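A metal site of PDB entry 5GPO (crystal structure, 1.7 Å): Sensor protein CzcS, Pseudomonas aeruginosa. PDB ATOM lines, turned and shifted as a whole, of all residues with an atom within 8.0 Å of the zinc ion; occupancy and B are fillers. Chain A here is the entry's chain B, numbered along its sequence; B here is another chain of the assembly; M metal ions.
ND1 of His 39 of chain B is in hydrogen-bond range of O of Ala 35 of chain B (2.8 Å). The side-chain amide nitrogen (NE2) of Gln 42 of chain B lies within hydrogen-bond range of the side-chain carboxylate (OD1) of Asp 43 (2.8 Å).
Within 4 Å of the zinc ion: His 39 of chain A, Asp 43 and His 39 of chain B.
NE2 of His 39 of chain A binds the zinc ion, 1.9 Å away. NE2 of His 39 of chain B is bound to the zinc ion. The zinc ion is bound by the side-chain carboxylate (OD2) of Asp 43, at 2.1 Å.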
ATOM      1  N   HIS A  39      -1.911 -19.339   1.450  1.00  0.00           N
ATOM      2  CA  HIS A  39      -2.248 -18.366   0.413  1.00  0.00           C
ATOM      3  C   HIS A  39      -0.999 -17.842  -0.292  1.00  0.00           C
ATOM      4  O   HIS A  39      -0.997 -17.652  -1.513  1.00  0.00           O
ATOM      5  CB  HIS A  39      -3.031 -17.220   1.034  1.00  0.00           C
ATOM      6  CG  HIS A  39      -3.494 -16.220   0.039  1.00  0.00           C
ATOM      7  ND1 HIS A  39      -4.717 -16.323  -0.604  1.00  0.00           N
ATOM      8  CD2 HIS A  39      -2.903 -15.115  -0.460  1.00  0.00           C
ATOM      9  CE1 HIS A  39      -4.858 -15.318  -1.441  1.00  0.00           C
ATOM     10  NE2 HIS A  39      -3.765 -14.562  -1.380  1.00  0.00           N
ATOM     11  N   ALA A  40       0.077 -17.601   0.463  1.00  0.00           N
ATOM     12  CA  ALA A  40       1.311 -17.130  -0.154  1.00  0.00           C
ATOM     13  C   ALA A  40       1.911 -18.166  -1.096  1.00  0.00           C
ATOM     14  O   ALA A  40       2.380 -17.826  -2.185  1.00  0.00           O
ATOM     15  CB  ALA A  40       2.318 -16.744   0.933  1.00  0.00           C
ATOM     16  N   GLN A  42       0.309 -20.560  -2.696  1.00  0.00           N
ATOM     17  CA  GLN A  42      -0.527 -20.698  -3.882  1.00  0.00           C
ATOM     18  C   GLN A  42      -0.318 -19.539  -4.848  1.00  0.00           C
ATOM     19  O   GLN A  42      -0.263 -19.742  -6.066  1.00  0.00           O
ATOM     20  CB  GLN A  42      -1.996 -20.807  -3.471  1.00  0.00           C
ATOM     21  CG  GLN A  42      -3.011 -20.920  -4.634  1.00  0.00           C
ATOM     22  CD  GLN A  42      -2.959 -22.250  -5.384  1.00  0.00           C
ATOM     23  OE1 GLN A  42      -1.884 -22.784  -5.660  1.00  0.00           O
ATOM     24  NE2 GLN A  42      -4.121 -22.799  -5.706  1.00  0.00           N
ATOM     25  N   ASP A  43      -0.142 -18.324  -4.323  1.00  0.00           N
ATOM     26  CA  ASP A  43       0.120 -17.194  -5.209  1.00  0.00           C
ATOM     27  C   ASP A  43       1.470 -17.353  -5.905  1.00  0.00           C
ATOM     28  O   ASP A  43       1.607 -17.006  -7.079  1.00  0.00           O
ATOM     29  CB  ASP A  43       0.049 -15.870  -4.444  1.00  0.00           C
ATOM     30  CG  ASP A  43      -1.380 -15.397  -4.254  1.00  0.00           C
ATOM     31  OD1 ASP A  43      -2.326 -16.192  -4.448  1.00  0.00           O
ATOM     32  OD2 ASP A  43      -1.556 -14.208  -3.904  1.00  0.00           O
ATOM     33  N   GLN A  44       2.460 -17.901  -5.205  1.00  0.00           N
ATOM     34  CA  GLN A  44       3.785 -18.043  -5.786  1.00  0.00           C
ATOM     35  C   GLN A  44       3.837 -19.167  -6.821  1.00  0.00           C
ATOM     36  O   GLN A  44       4.619 -19.083  -7.774  1.00  0.00           O
ATOM     37  CB  GLN A  44       4.826 -18.274  -4.699  1.00  0.00           C
ATOM     38  CG  GLN A  44       6.262 -18.382  -5.236  1.00  0.00           C
ATOM     39  CD  GLN A  44       6.876 -17.032  -5.604  1.00  0.00           C
ATOM     40  OE1 GLN A  44       6.217 -16.163  -6.185  1.00  0.00           O
ATOM     41  NE2 GLN A  44       8.148 -16.853  -5.265  1.00  0.00           N
ATOM     42  N   ALA B  35     -11.612  -9.585  -5.967  1.00  0.00           N
ATOM     43  CA  ALA B  35     -10.344 -10.202  -5.586  1.00  0.00           C
ATOM     44  C   ALA B  35     -10.512 -11.697  -5.367  1.00  0.00           C
ATOM     45  O   ALA B  35      -9.625 -12.489  -5.687  1.00  0.00           O
ATOM     46  CB  ALA B  35      -9.773  -9.542  -4.334  1.00  0.00           C
ATOM     47  N   ALA B  38     -10.942 -13.161  -8.784  1.00  0.00           N
ATOM     48  CA  ALA B  38      -9.634 -13.259  -9.434  1.00  0.00           C
ATOM     49  C   ALA B  38      -8.854 -14.448  -8.911  1.00  0.00           C
ATOM     50  O   ALA B  38      -8.212 -15.174  -9.692  1.00  0.00           O
ATOM     51  CB  ALA B  38      -8.854 -11.961  -9.248  1.00  0.00           C
ATOM     52  N   HIS B  39      -8.874 -14.667  -7.603  1.00  0.00           N
ATOM     53  CA  HIS B  39      -8.150 -15.813  -7.038  1.00  0.00           C
ATOM     54  C   HIS B  39      -8.756 -17.130  -7.492  1.00  0.00           C
ATOM     55  O   HIS B  39      -8.022 -18.114  -7.697  1.00  0.00           O
ATOM     56  CB  HIS B  39      -8.140 -15.726  -5.520  1.00  0.00           C
ATOM     57  CG  HIS B  39      -7.033 -14.874  -4.980  1.00  0.00           C
ATOM     58  ND1 HIS B  39      -7.194 -13.525  -4.728  1.00  0.00           N
ATOM     59  CD2 HIS B  39      -5.765 -15.180  -4.642  1.00  0.00           C
ATOM     60  CE1 HIS B  39      -6.057 -13.050  -4.258  1.00  0.00           C
ATOM     61  NE2 HIS B  39      -5.177 -14.026  -4.194  1.00  0.00           N
ATOM     62  N   GLN B  42      -7.281 -17.674 -10.856  1.00  0.00           N
ATOM     63  CA  GLN B  42      -5.939 -18.149 -10.581  1.00  0.00           C
ATOM     64  C   GLN B  42      -5.920 -19.647 -10.240  1.00  0.00           C
ATOM     65  O   GLN B  42      -5.102 -20.395 -10.768  1.00  0.00           O
ATOM     66  CB  GLN B  42      -5.348 -17.326  -9.439  1.00  0.00           C
ATOM     67  CG  GLN B  42      -3.966 -17.711  -9.040  1.00  0.00           C
ATOM     68  CD  GLN B  42      -3.340 -16.668  -8.142  1.00  0.00           C
ATOM     69  OE1 GLN B  42      -2.601 -15.791  -8.603  1.00  0.00           O
ATOM     70  NE2 GLN B  42      -3.645 -16.752  -6.852  1.00  0.00           N
HETATM   71 ZN    ZN M   1      -3.449 -13.735  -3.093  1.00  0.00          ZN
